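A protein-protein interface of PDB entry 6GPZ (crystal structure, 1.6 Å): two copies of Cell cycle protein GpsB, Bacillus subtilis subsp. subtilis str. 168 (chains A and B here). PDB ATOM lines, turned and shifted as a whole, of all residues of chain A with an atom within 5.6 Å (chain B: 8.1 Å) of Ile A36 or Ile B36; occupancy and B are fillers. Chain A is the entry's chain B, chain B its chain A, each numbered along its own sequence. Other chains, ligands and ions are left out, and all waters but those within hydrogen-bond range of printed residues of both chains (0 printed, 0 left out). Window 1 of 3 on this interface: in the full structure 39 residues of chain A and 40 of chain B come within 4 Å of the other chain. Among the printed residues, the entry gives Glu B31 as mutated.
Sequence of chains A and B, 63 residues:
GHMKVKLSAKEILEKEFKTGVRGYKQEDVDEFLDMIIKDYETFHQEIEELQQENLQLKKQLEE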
ATOM      1  N   LEU A   7      25.908  20.263 -20.793  1.00  0.00           N
ATOM      2  CA  LEU A   7      25.765  19.108 -19.903  1.00  0.00           C
ATOM      3  C   LEU A   7      27.101  18.452 -19.594  1.00  0.00           C
ATOM      4  O   LEU A   7      28.124  18.678 -20.231  1.00  0.00           O
ATOM      5  CB  LEU A   7      24.837  18.059 -20.568  1.00  0.00           C
ATOM      6  CG  LEU A   7      23.417  18.497 -20.880  1.00  0.00           C
ATOM      7  CD1 LEU A   7      22.607  17.515 -21.748  1.00  0.00           C
ATOM      8  CD2 LEU A   7      22.697  18.690 -19.521  1.00  0.00           C
ATOM      9  N   ILE A  12      24.073  13.656 -17.229  1.00  0.00           N
ATOM     10  CA  ILE A  12      23.282  12.717 -18.051  1.00  0.00           C
ATOM     11  C   ILE A  12      23.046  11.404 -17.303  1.00  0.00           C
ATOM     12  O   ILE A  12      21.952  10.820 -17.369  1.00  0.00           O
ATOM     13  CB  ILE A  12      23.996  12.498 -19.388  1.00  0.00           C
ATOM     14  CG1 ILE A  12      24.031  13.836 -20.144  1.00  0.00           C
ATOM     15  CG2 ILE A  12      23.202  11.440 -20.244  1.00  0.00           C
ATOM     16  CD1 ILE A  12      24.902  13.807 -21.396  1.00  0.00           C
ATOM     17  N   PHE A  32      20.765   3.866 -24.395  1.00  0.00           N
ATOM     18  CA  PHE A  32      21.294   4.798 -25.383  1.00  0.00           C
ATOM     19  C   PHE A  32      22.009   5.955 -24.698  1.00  0.00           C
ATOM     20  O   PHE A  32      23.095   6.392 -25.166  1.00  0.00           O
ATOM     21  CB  PHE A  32      20.140   5.312 -26.212  1.00  0.00           C
ATOM     22  CG  PHE A  32      20.557   6.089 -27.429  1.00  0.00           C
ATOM     23  CD1 PHE A  32      20.262   7.405 -27.529  1.00  0.00           C
ATOM     24  CD2 PHE A  32      21.194   5.447 -28.439  1.00  0.00           C
ATOM     25  CE1 PHE A  32      20.606   8.116 -28.715  1.00  0.00           C
ATOM     26  CE2 PHE A  32      21.529   6.095 -29.618  1.00  0.00           C
ATOM     27  CZ  PHE A  32      21.231   7.457 -29.747  1.00  0.00           C
ATOM     28  N   LEU A  33      21.424   6.460 -23.598  1.00  0.00           N
ATOM     29  CA  LEU A  33      22.108   7.493 -22.828  1.00  0.00           C
ATOM     30  C   LEU A  33      23.420   6.964 -22.277  1.00  0.00           C
ATOM     31  O   LEU A  33      24.382   7.741 -22.167  1.00  0.00           O
ATOM     32  CB  LEU A  33      21.193   8.024 -21.717  1.00  0.00           C
ATOM     33  CG  LEU A  33      20.064   8.955 -22.188  1.00  0.00           C
ATOM     34  CD1 LEU A  33      19.203   9.391 -20.998  1.00  0.00           C
ATOM     35  CD2 LEU A  33      20.571  10.189 -22.926  1.00  0.00           C
ATOM     36  N   ASP A  34      23.525   5.657 -21.982  1.00  0.00           N
ATOM     37  CA  ASP A  34      24.812   5.167 -21.479  1.00  0.00           C
ATOM     38  C   ASP A  34      25.900   5.317 -22.538  1.00  0.00           C
ATOM     39  O   ASP A  34      27.065   5.557 -22.202  1.00  0.00           O
ATOM     40  CB  ASP A  34      24.672   3.707 -21.050  1.00  0.00           C
ATOM     41  CG  ASP A  34      23.982   3.550 -19.690  1.00  0.00           C
ATOM     42  OD1 ASP A  34      23.418   2.452 -19.418  1.00  0.00           O
ATOM     43  OD2 ASP A  34      24.006   4.491 -18.901  1.00  0.00           O
ATOM     44  N   MET A  35      25.543   5.146 -23.807  1.00  0.00           N
ATOM     45  CA  MET A  35      26.517   5.326 -24.883  1.00  0.00           C
ATOM     46  C   MET A  35      26.908   6.779 -24.994  1.00  0.00           C
ATOM     47  O   MET A  35      28.082   7.080 -25.218  1.00  0.00           O
ATOM     48  CB  MET A  35      25.954   4.837 -26.213  1.00  0.00           C
ATOM     49  CG  MET A  35      25.792   3.324 -26.221  1.00  0.00           C
ATOM     50  SD  MET A  35      25.183   2.855 -27.860  1.00  0.00           S
ATOM     51  CE  MET A  35      23.473   3.163 -27.670  1.00  0.00           C
ATOM     52  N   ILE A  36      25.930   7.678 -24.853  1.00  0.00           N
ATOM     53  CA  ILE A  36      26.194   9.131 -24.844  1.00  0.00           C
ATOM     54  C   ILE A  36      27.130   9.500 -23.705  1.00  0.00           C
ATOM     55  O   ILE A  36      28.038  10.332 -23.876  1.00  0.00           O
ATOM     56  CB  ILE A  36      24.862   9.894 -24.788  1.00  0.00           C
ATOM     57  CG1 ILE A  36      24.143   9.737 -26.134  1.00  0.00           C
ATOM     58  CG2 ILE A  36      25.089  11.438 -24.495  1.00  0.00           C
ATOM     59  CD1 ILE A  36      22.684  10.192 -26.225  1.00  0.00           C
ATOM     60  N   ILE A  37      26.910   8.938 -22.519  1.00  0.00           N
ATOM     61  CA  ILE A  37      27.763   9.247 -21.373  1.00  0.00           C
ATOM     62  C   ILE A  37      29.213   8.909 -21.689  1.00  0.00           C
ATOM     63  O   ILE A  37      30.140   9.689 -21.394  1.00  0.00           O
ATOM     64  CB  ILE A  37      27.233   8.479 -20.141  1.00  0.00           C
ATOM     65  CG1 ILE A  37      25.965   9.168 -19.663  1.00  0.00           C
ATOM     66  CG2 ILE A  37      28.293   8.421 -19.083  1.00  0.00           C
ATOM     67  CD1 ILE A  37      25.091   8.323 -18.729  1.00  0.00           C
ATOM     68  N   LYS A  38      29.445   7.764 -22.309  1.00  0.00           N
ATOM     69  CA  LYS A  38      30.830   7.393 -22.607  1.00  0.00           C
ATOM     70  C   LYS A  38      31.435   8.361 -23.614  1.00  0.00           C
ATOM     71  O   LYS A  38      32.621   8.695 -23.527  1.00  0.00           O
ATOM     72  CB  LYS A  38      30.881   5.960 -23.157  1.00  0.00           C
ATOM     73  CG  LYS A  38      30.581   4.879 -22.126  1.00  0.00           C
ATOM     74  N   ASP A  39      30.625   8.840 -24.575  1.00  0.00           N
ATOM     75  CA  ASP A  39      31.122   9.855 -25.520  1.00  0.00           C
ATOM     76  C   ASP A  39      31.444  11.162 -24.802  1.00  0.00           C
ATOM     77  O   ASP A  39      32.481  11.789 -25.064  1.00  0.00           O
ATOM     78  CB  ASP A  39      30.087  10.097 -26.623  1.00  0.00           C
ATOM     79  CG  ASP A  39      30.131   9.054 -27.723  1.00  0.00           C
ATOM     80  OD1 ASP A  39      31.023   8.154 -27.705  1.00  0.00           O
ATOM     81  OD2 ASP A  39      29.229   9.126 -28.617  1.00  0.00           O
ATOM     82  N   TYR A  40      30.578  11.618 -23.908  1.00  0.00           N
ATOM     83  CA  TYR A  40      30.953  12.806 -23.123  1.00  0.00           C
ATOM     84  C   TYR A  40      32.289  12.598 -22.402  1.00  0.00           C
ATOM     85  O   TYR A  40      33.107  13.521 -22.363  1.00  0.00           O
ATOM     86  CB  TYR A  40      29.869  13.175 -22.099  1.00  0.00           C
ATOM     87  CG  TYR A  40      28.801  14.118 -22.611  1.00  0.00           C
ATOM     88  CD1 TYR A  40      27.883  13.729 -23.597  1.00  0.00           C
ATOM     89  CD2 TYR A  40      28.682  15.413 -22.100  1.00  0.00           C
ATOM     90  CE1 TYR A  40      26.895  14.588 -24.022  1.00  0.00           C
ATOM     91  CE2 TYR A  40      27.704  16.305 -22.561  1.00  0.00           C
ATOM     92  CZ  TYR A  40      26.793  15.851 -23.528  1.00  0.00           C
ATOM     93  OH  TYR A  40      25.794  16.696 -23.937  1.00  0.00           O
ATOM     94  N   GLU A  41      32.518  11.409 -21.819  1.00  0.00           N
ATOM     95  CA  GLU A  41      33.783  11.158 -21.129  1.00  0.00           C
ATOM     96  C   GLU A  41      34.957  11.211 -22.110  1.00  0.00           C
ATOM     97  O   GLU A  41      36.011  11.803 -21.794  1.00  0.00           O
ATOM     98  CB  GLU A  41      33.695   9.814 -20.356  1.00  0.00           C
ATOM     99  CG  GLU A  41      32.572   9.870 -19.322  1.00  0.00           C
ATOM    100  CD  GLU A  41      32.448   8.643 -18.465  1.00  0.00           C
ATOM    101  OE1 GLU A  41      32.825   7.558 -18.945  1.00  0.00           O
ATOM    102  OE2 GLU A  41      31.954   8.765 -17.318  1.00  0.00           O
ATOM    103  N   LYS B   6      31.245   6.929 -29.990  1.00  0.00           N
ATOM    104  CA  LYS B   6      30.258   5.900 -30.349  1.00  0.00           C
ATOM    105  C   LYS B   6      29.179   6.419 -31.283  1.00  0.00           C
ATOM    106  O   LYS B   6      28.679   5.675 -32.140  1.00  0.00           O
ATOM    107  CB  LYS B   6      29.580   5.361 -29.082  1.00  0.00           C
ATOM    108  CG  LYS B   6      30.440   4.339 -28.356  1.00  0.00           C
ATOM    109  CD  LYS B   6      30.155   4.236 -26.867  1.00  0.00           C
ATOM    110  CE  LYS B   6      31.145   3.237 -26.264  1.00  0.00           C
ATOM    111  NZ  LYS B   6      31.056   1.888 -26.949  1.00  0.00           N
ATOM    112  N   LEU B   7      28.774   7.668 -31.115  1.00  0.00           N
ATOM    113  CA  LEU B   7      27.583   8.197 -31.779  1.00  0.00           C
ATOM    114  C   LEU B   7      27.892   9.522 -32.454  1.00  0.00           C
ATOM    115  O   LEU B   7      28.982  10.063 -32.367  1.00  0.00           O
ATOM    116  CB  LEU B   7      26.395   8.428 -30.815  1.00  0.00           C
ATOM    117  CG  LEU B   7      25.927   7.203 -30.086  1.00  0.00           C
ATOM    118  CD1 LEU B   7      24.995   7.636 -28.975  1.00  0.00           C
ATOM    119  CD2 LEU B   7      25.169   6.346 -31.097  1.00  0.00           C
ATOM    120  N   SER B   8      26.917   9.999 -33.215  1.00  0.00           N
ATOM    121  CA  SER B   8      27.016  11.246 -33.940  1.00  0.00           C
ATOM    122  C   SER B   8      25.718  11.954 -33.718  1.00  0.00           C
ATOM    123  O   SER B   8      24.739  11.338 -33.320  1.00  0.00           O
ATOM    124  CB  SER B   8      27.237  11.037 -35.431  1.00  0.00           C
ATOM    125  OG  SER B   8      26.088  10.511 -36.047  1.00  0.00           O
ATOM    126  N   ALA B   9      25.694  13.246 -33.979  1.00  0.00           N
ATOM    127  CA  ALA B   9      24.439  13.974 -33.816  1.00  0.00           C
ATOM    128  C   ALA B   9      23.358  13.384 -34.718  1.00  0.00           C
ATOM    129  O   ALA B   9      22.195  13.273 -34.315  1.00  0.00           O
ATOM    130  CB  ALA B   9      24.632  15.444 -34.157  1.00  0.00           C
ATOM    131  N   GLU B  11      23.056  10.233 -35.702  1.00  0.00           N
ATOM    132  CA  GLU B  11      22.558   8.980 -35.117  1.00  0.00           C
ATOM    133  C   GLU B  11      21.613   9.242 -33.956  1.00  0.00           C
ATOM    134  O   GLU B  11      20.635   8.498 -33.732  1.00  0.00           O
ATOM    135  CB  GLU B  11      23.756   8.118 -34.680  1.00  0.00           C
ATOM    136  CG  GLU B  11      24.409   7.481 -35.928  1.00  0.00           C
ATOM    137  CD  GLU B  11      25.661   6.660 -35.647  1.00  0.00           C
ATOM    138  OE1 GLU B  11      25.851   5.621 -36.318  1.00  0.00           O
ATOM    139  OE2 GLU B  11      26.471   7.062 -34.793  1.00  0.00           O
ATOM    140  N   ILE B  12      21.851  10.322 -33.234  1.00  0.00           N
ATOM    141  CA  ILE B  12      20.945  10.642 -32.132  1.00  0.00           C
ATOM    142  C   ILE B  12      19.591  11.119 -32.667  1.00  0.00           C
ATOM    143  O   ILE B  12      18.534  10.747 -32.180  1.00  0.00           O
ATOM    144  CB  ILE B  12      21.600  11.695 -31.217  1.00  0.00           C
ATOM    145  CG1 ILE B  12      22.843  11.070 -30.604  1.00  0.00           C
ATOM    146  CG2 ILE B  12      20.626  12.157 -30.136  1.00  0.00           C
ATOM    147  CD1 ILE B  12      23.849  12.044 -29.817  1.00  0.00           C
ATOM    148  N   LYS B  15      17.666   7.926 -33.988  1.00  0.00           N
ATOM    149  CA  LYS B  15      17.320   6.867 -33.036  1.00  0.00           C
ATOM    150  C   LYS B  15      15.846   6.872 -32.693  1.00  0.00           C
ATOM    151  O   LYS B  15      15.247   7.930 -32.461  1.00  0.00           O
ATOM    152  CB  LYS B  15      18.133   7.100 -31.758  1.00  0.00           C
ATOM    153  CG  LYS B  15      17.793   6.098 -30.627  1.00  0.00           C
ATOM    154  CD  LYS B  15      18.158   4.680 -30.976  1.00  0.00           C
ATOM    155  CE  LYS B  15      17.925   3.835 -29.670  1.00  0.00           C
ATOM    156  NZ  LYS B  15      18.259   2.413 -30.023  1.00  0.00           N
ATOM    157  N   PHE B  17      12.869   4.922 -30.159  1.00  0.00           N
ATOM    158  CA  PHE B  17      12.671   4.111 -28.970  1.00  0.00           C
ATOM    159  C   PHE B  17      11.303   3.457 -29.024  1.00  0.00           C
ATOM    160  O   PHE B  17      10.331   4.096 -29.406  1.00  0.00           O
ATOM    161  CB  PHE B  17      12.744   5.020 -27.688  1.00  0.00           C
ATOM    162  CG  PHE B  17      13.960   5.872 -27.641  1.00  0.00           C
ATOM    163  CD1 PHE B  17      15.170   5.343 -27.236  1.00  0.00           C
ATOM    164  CD2 PHE B  17      13.886   7.237 -27.966  1.00  0.00           C
ATOM    165  CE1 PHE B  17      16.313   6.132 -27.200  1.00  0.00           C
ATOM    166  CE2 PHE B  17      15.066   8.062 -28.006  1.00  0.00           C
ATOM    167  CZ  PHE B  17      16.261   7.501 -27.546  1.00  0.00           C
ATOM    168  N   VAL B  29      12.398  13.584 -22.831  1.00  0.00           N
ATOM    169  CA  VAL B  29      13.549  12.902 -23.407  1.00  0.00           C
ATOM    170  C   VAL B  29      14.009  13.635 -24.667  1.00  0.00           C
ATOM    171  O   VAL B  29      15.206  13.870 -24.846  1.00  0.00           O
ATOM    172  CB  VAL B  29      13.215  11.439 -23.742  1.00  0.00           C
ATOM    173  CG1 VAL B  29      14.419  10.764 -24.547  1.00  0.00           C
ATOM    174  CG2 VAL B  29      12.903  10.678 -22.418  1.00  0.00           C
ATOM    175  N   ASP B  30      13.077  13.996 -25.547  1.00  0.00           N
ATOM    176  CA  ASP B  30      13.495  14.613 -26.824  1.00  0.00           C
ATOM    177  C   ASP B  30      14.204  15.949 -26.559  1.00  0.00           C
ATOM    178  O   ASP B  30      15.161  16.324 -27.259  1.00  0.00           O
ATOM    179  CB  ASP B  30      12.294  14.901 -27.732  1.00  0.00           C
ATOM    180  CG  ASP B  30      11.643  13.698 -28.327  1.00  0.00           C
ATOM    181  OD1 ASP B  30      12.214  12.581 -28.258  1.00  0.00           O
ATOM    182  OD2 ASP B  30      10.553  13.900 -28.911  1.00  0.00           O
ATOM    183  N   GLU B  31      13.686  16.746 -25.603  1.00  0.00           N
ATOM    184  CA  GLU B  31      14.294  18.046 -25.360  1.00  0.00           C
ATOM    185  C   GLU B  31      15.666  17.896 -24.741  1.00  0.00           C
ATOM    186  O   GLU B  31      16.570  18.727 -25.008  1.00  0.00           O
ATOM    187  CB  GLU B  31      13.364  18.913 -24.484  1.00  0.00           C
ATOM    188  CG  GLU B  31      12.127  19.396 -25.293  1.00  0.00           C
ATOM    189  CD  GLU B  31      11.023  20.006 -24.465  1.00  0.00           C
ATOM    190  OE1 GLU B  31       9.971  20.339 -25.067  1.00  0.00           O
ATOM    191  OE2 GLU B  31      11.205  20.200 -23.250  1.00  0.00           O
ATOM    192  N   PHE B  32      15.871  16.808 -23.986  1.00  0.00           N
ATOM    193  CA  PHE B  32      17.209  16.538 -23.436  1.00  0.00           C
ATOM    194  C   PHE B  32      18.160  16.106 -24.543  1.00  0.00           C
ATOM    195  O   PHE B  32      19.322  16.551 -24.573  1.00  0.00           O
ATOM    196  CB  PHE B  32      17.091  15.442 -22.382  1.00  0.00           C
ATOM    197  CG  PHE B  32      18.265  15.365 -21.413  1.00  0.00           C
ATOM    198  CD1 PHE B  32      18.573  16.406 -20.599  1.00  0.00           C
ATOM    199  CD2 PHE B  32      19.023  14.201 -21.346  1.00  0.00           C
ATOM    200  CE1 PHE B  32      19.657  16.308 -19.710  1.00  0.00           C
ATOM    201  CE2 PHE B  32      20.109  14.096 -20.487  1.00  0.00           C
ATOM    202  CZ  PHE B  32      20.391  15.152 -19.638  1.00  0.00           C
ATOM    203  N   LEU B  33      17.658  15.288 -25.480  1.00  0.00           N
ATOM    204  CA  LEU B  33      18.465  14.903 -26.661  1.00  0.00           C
ATOM    205  C   LEU B  33      18.852  16.123 -27.474  1.00  0.00           C
ATOM    206  O   LEU B  33      19.964  16.153 -28.053  1.00  0.00           O
ATOM    207  CB  LEU B  33      17.724  13.891 -27.554  1.00  0.00           C
ATOM    208  CG  LEU B  33      17.521  12.551 -26.836  1.00  0.00           C
ATOM    209  CD1 LEU B  33      16.686  11.609 -27.636  1.00  0.00           C
ATOM    210  CD2 LEU B  33      18.862  11.847 -26.561  1.00  0.00           C
ATOM    211  N   ASP B  34      17.980  17.140 -27.530  1.00  0.00           N
ATOM    212  CA  ASP B  34      18.329  18.336 -28.315  1.00  0.00           C
ATOM    213  C   ASP B  34      19.530  19.005 -27.710  1.00  0.00           C
ATOM    214  O   ASP B  34      20.410  19.460 -28.435  1.00  0.00           O
ATOM    215  CB  ASP B  34      17.130  19.314 -28.339  1.00  0.00           C
ATOM    216  CG  ASP B  34      17.479  20.670 -28.948  1.00  0.00           C
ATOM    217  OD1 ASP B  34      17.498  21.689 -28.209  1.00  0.00           O
ATOM    218  OD2 ASP B  34      17.726  20.688 -30.173  1.00  0.00           O
ATOM    219  N   MET B  35      19.571  19.089 -26.387  1.00  0.00           N
ATOM    220  CA  MET B  35      20.715  19.696 -25.724  1.00  0.00           C
ATOM    221  C   MET B  35      21.983  18.913 -26.008  1.00  0.00           C
ATOM    222  O   MET B  35      23.082  19.495 -26.180  1.00  0.00           O
ATOM    223  CB  MET B  35      20.447  19.727 -24.203  1.00  0.00           C
ATOM    224  CG  MET B  35      19.363  20.692 -23.941  1.00  0.00           C
ATOM    225  SD  MET B  35      18.863  20.701 -22.204  1.00  0.00           S
ATOM    226  CE  MET B  35      17.559  21.960 -22.239  1.00  0.00           C
ATOM    227  N   ILE B  36      21.861  17.598 -25.943  1.00  0.00           N
ATOM    228  CA  ILE B  36      22.971  16.689 -26.209  1.00  0.00           C
ATOM    229  C   ILE B  36      23.504  16.898 -27.639  1.00  0.00           C
ATOM    230  O   ILE B  36      24.715  16.926 -27.853  1.00  0.00           O
ATOM    231  CB  ILE B  36      22.525  15.236 -25.951  1.00  0.00           C
ATOM    232  CG1 ILE B  36      22.408  15.048 -24.414  1.00  0.00           C
ATOM    233  CG2 ILE B  36      23.569  14.304 -26.558  1.00  0.00           C
ATOM    234  CD1 ILE B  36      21.658  13.740 -24.032  1.00  0.00           C
ATOM    235  N   ILE B  37      22.624  16.914 -28.651  1.00  0.00           N
ATOM    236  CA  ILE B  37      23.055  17.129 -30.042  1.00  0.00           C
ATOM    237  C   ILE B  37      23.836  18.429 -30.143  1.00  0.00           C
ATOM    238  O   ILE B  37      24.861  18.513 -30.832  1.00  0.00           O
ATOM    239  CB  ILE B  37      21.825  17.146 -30.979  1.00  0.00           C
ATOM    240  CG1 ILE B  37      21.307  15.703 -31.208  1.00  0.00           C
ATOM    241  CG2 ILE B  37      22.130  17.834 -32.343  1.00  0.00           C
ATOM    242  CD1 ILE B  37      19.898  15.695 -31.811  1.00  0.00           C
ATOM    243  N   LYS B  38      23.343  19.467 -29.478  1.00  0.00           N
ATOM    244  CA  LYS B  38      24.038  20.742 -29.525  1.00  0.00           C
ATOM    245  C   LYS B  38      25.423  20.636 -28.873  1.00  0.00           C
ATOM    246  O   LYS B  38      26.410  21.217 -29.393  1.00  0.00           O
ATOM    247  CB  LYS B  38      23.186  21.812 -28.856  1.00  0.00           C
ATOM    248  CG  LYS B  38      22.084  22.311 -29.819  1.00  0.00           C
ATOM    249  CD  LYS B  38      20.929  22.955 -29.084  1.00  0.00           C
ATOM    250  CE  LYS B  38      19.812  23.394 -30.041  1.00  0.00           C
ATOM    251  NZ  LYS B  38      18.609  23.819 -29.234  1.00  0.00           N
ATOM    252  N   ASP B  39      25.545  19.841 -27.805  1.00  0.00           N
ATOM    253  CA  ASP B  39      26.861  19.627 -27.173  1.00  0.00           C
ATOM    254  C   ASP B  39      27.814  18.834 -28.068  1.00  0.00           C
ATOM    255  O   ASP B  39      29.022  19.117 -28.093  1.00  0.00           O
ATOM    256  CB  ASP B  39      26.749  18.913 -25.820  1.00  0.00           C
ATOM    257  CG  ASP B  39      26.284  19.820 -24.691  1.00  0.00           C
ATOM    258  OD1 ASP B  39      26.052  19.311 -23.565  1.00  0.00           O
ATOM    259  OD2 ASP B  39      26.201  21.083 -24.863  1.00  0.00           O
ATOM    260  N   TYR B  40      27.323  17.810 -28.773  1.00  0.00           N
ATOM    261  CA  TYR B  40      28.216  17.098 -29.699  1.00  0.00           C
ATOM    262  C   TYR B  40      28.843  18.077 -30.693  1.00  0.00           C
ATOM    263  O   TYR B  40      30.016  17.948 -31.025  1.00  0.00           O
ATOM    264  CB  TYR B  40      27.476  15.990 -30.462  1.00  0.00           C
ATOM    265  CG  TYR B  40      27.482  14.607 -29.807  1.00  0.00           C
ATOM    266  CD1 TYR B  40      26.778  14.371 -28.606  1.00  0.00           C
ATOM    267  CD2 TYR B  40      28.139  13.536 -30.390  1.00  0.00           C
ATOM    268  CE1 TYR B  40      26.734  13.125 -28.031  1.00  0.00           C
ATOM    269  CE2 TYR B  40      28.113  12.281 -29.802  1.00  0.00           C
ATOM    270  CZ  TYR B  40      27.413  12.081 -28.607  1.00  0.00           C
ATOM    271  OH  TYR B  40      27.341  10.849 -28.000  1.00  0.00           O
ATOM    272  N   GLU B  41      28.057  19.033 -31.186  1.00  0.00           N
ATOM    273  CA  GLU B  41      28.569  20.052 -32.116  1.00  0.00           C
ATOM    274  C   GLU B  41      29.627  20.920 -31.454  1.00  0.00           C
ATOM    275  O   GLU B  41      30.691  21.197 -32.039  1.00  0.00           O
ATOM    276  CB  GLU B  41      27.378  20.891 -32.583  1.00  0.00           C
ATOM    277  CG  GLU B  41      27.763  22.161 -33.336  1.00  0.00           C
ATOM    278  N   THR B  42      29.344  21.368 -30.234  1.00  0.00           N
ATOM    279  CA  THR B  42      30.305  22.168 -29.479  1.00  0.00           C
ATOM    280  C   THR B  42      31.595  21.404 -29.210  1.00  0.00           C
ATOM    281  O   THR B  42      32.686  21.932 -29.459  1.00  0.00           O
ATOM    282  CB  THR B  42      29.669  22.657 -28.179  1.00  0.00           C
ATOM    283  OG1 THR B  42      28.514  23.433 -28.515  1.00  0.00           O
ATOM    284  CG2 THR B  42      30.627  23.535 -27.388  1.00  0.00           C
ATOM    285  N   PHE B  43      31.494  20.177 -28.697  1.00  0.00           N
ATOM    286  CA  PHE B  43      32.693  19.366 -28.483  1.00  0.00           C
ATOM    287  C   PHE B  43      33.522  19.247 -29.751  1.00  0.00           C
ATOM    288  O   PHE B  43      34.758  19.352 -29.722  1.00  0.00           O
ATOM    289  CB  PHE B  43      32.300  17.953 -28.035  1.00  0.00           C
ATOM    290  CG  PHE B  43      31.964  17.817 -26.575  1.00  0.00           C
ATOM    291  CD1 PHE B  43      32.784  18.282 -25.568  1.00  0.00           C
ATOM    292  CD2 PHE B  43      30.788  17.111 -26.255  1.00  0.00           C
ATOM    293  CE1 PHE B  43      32.437  18.082 -24.227  1.00  0.00           C
ATOM    294  CE2 PHE B  43      30.429  16.877 -24.971  1.00  0.00           C
ATOM    295  CZ  PHE B  43      31.218  17.385 -23.941  1.00  0.00           C
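Leu A7 touches Phe B32, and with the chains exchanged Phe A32 touches Leu B7.
Leu A7 touches Asp B39, and with the chains exchanged Asp A39 touches Leu B7.
Ile A12 touches Phe B32, and with the chains exchanged Phe A32 touches Ile B12.
Asp A39 touches Tyr B40, and with the chains exchanged Tyr A40 touches Asp B39.
Positions printed for both chains: 7, 12, 32, 33, 34, 35, 36, 37, 38, 39, 40 and 41.
Of the 19 pairs that touch across the chains among the printed residues, 13 have their exchanged pair printed and touching as well.
Phe B32 touches Leu A7 (CE1 to CD1, 3.8 Å).
Leu A7 touches Met B35 (CD1 to CB, 3.9 Å).
CD1 of Leu A7 touches CG1 of Ile B36, 3.6 Å away.
Phe A32 touches Leu B7.
Phe A32 touches Ile B12.
CD2 of Leu A33 touches CD1 of Ile B36 (3.9 Å).
CG1 of Ile A36 touches CD1 of Leu B7, 3.6 Å away.
CG2 of Ile A36 touches CG2 of Ile B36, at 3.8 Å.
Tyr A40 touches Ile B36.
Tyr A40 touches Phe B43.
OD1 of Asp B39 sits at hydrogen-bond distance from N of Leu A7 (2.9 Å).
N of Lys B6 is in hydrogen-bond range of OD1 of Asp A39 (2.6 Å).
N of Leu B7 lies within hydrogen-bond range of OD2 of Asp A39 (2.9 Å).
The side-chain hydroxyl of Tyr B40 lies within hydrogen-bond range of the side-chain carboxylate of Asp A39, at 2.6 Å.
OD1 of Asp B39 sits at hydrogen-bond distance from OH of Tyr A40, 2.7 Å away.
Of the 12 printed residues of chain A, 8 touch a printed residue of chain B.
Of the printed residues of chain B, Ile A12 touches Phe B32 (3.9 Å).
Ile A36 touches just these residues of chain B: Leu B7, Ile B36 and Tyr B40.
Of the printed residues of chain A, Ile B36 touches Leu A7, Leu A33, Ile A36 and Tyr A40.
Of the printed residues of chain A, Asp B39 touches Leu A7 and Tyr A40.
Thr B42 touches none of the printed residues of chain A.
The nearest printed residue of chain B that does not touch Ile A36 is Leu B33 (4.2 Å).
The nearest printed residue of chain B that does not touch Leu A7 is Phe B43 (5.0 Å).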
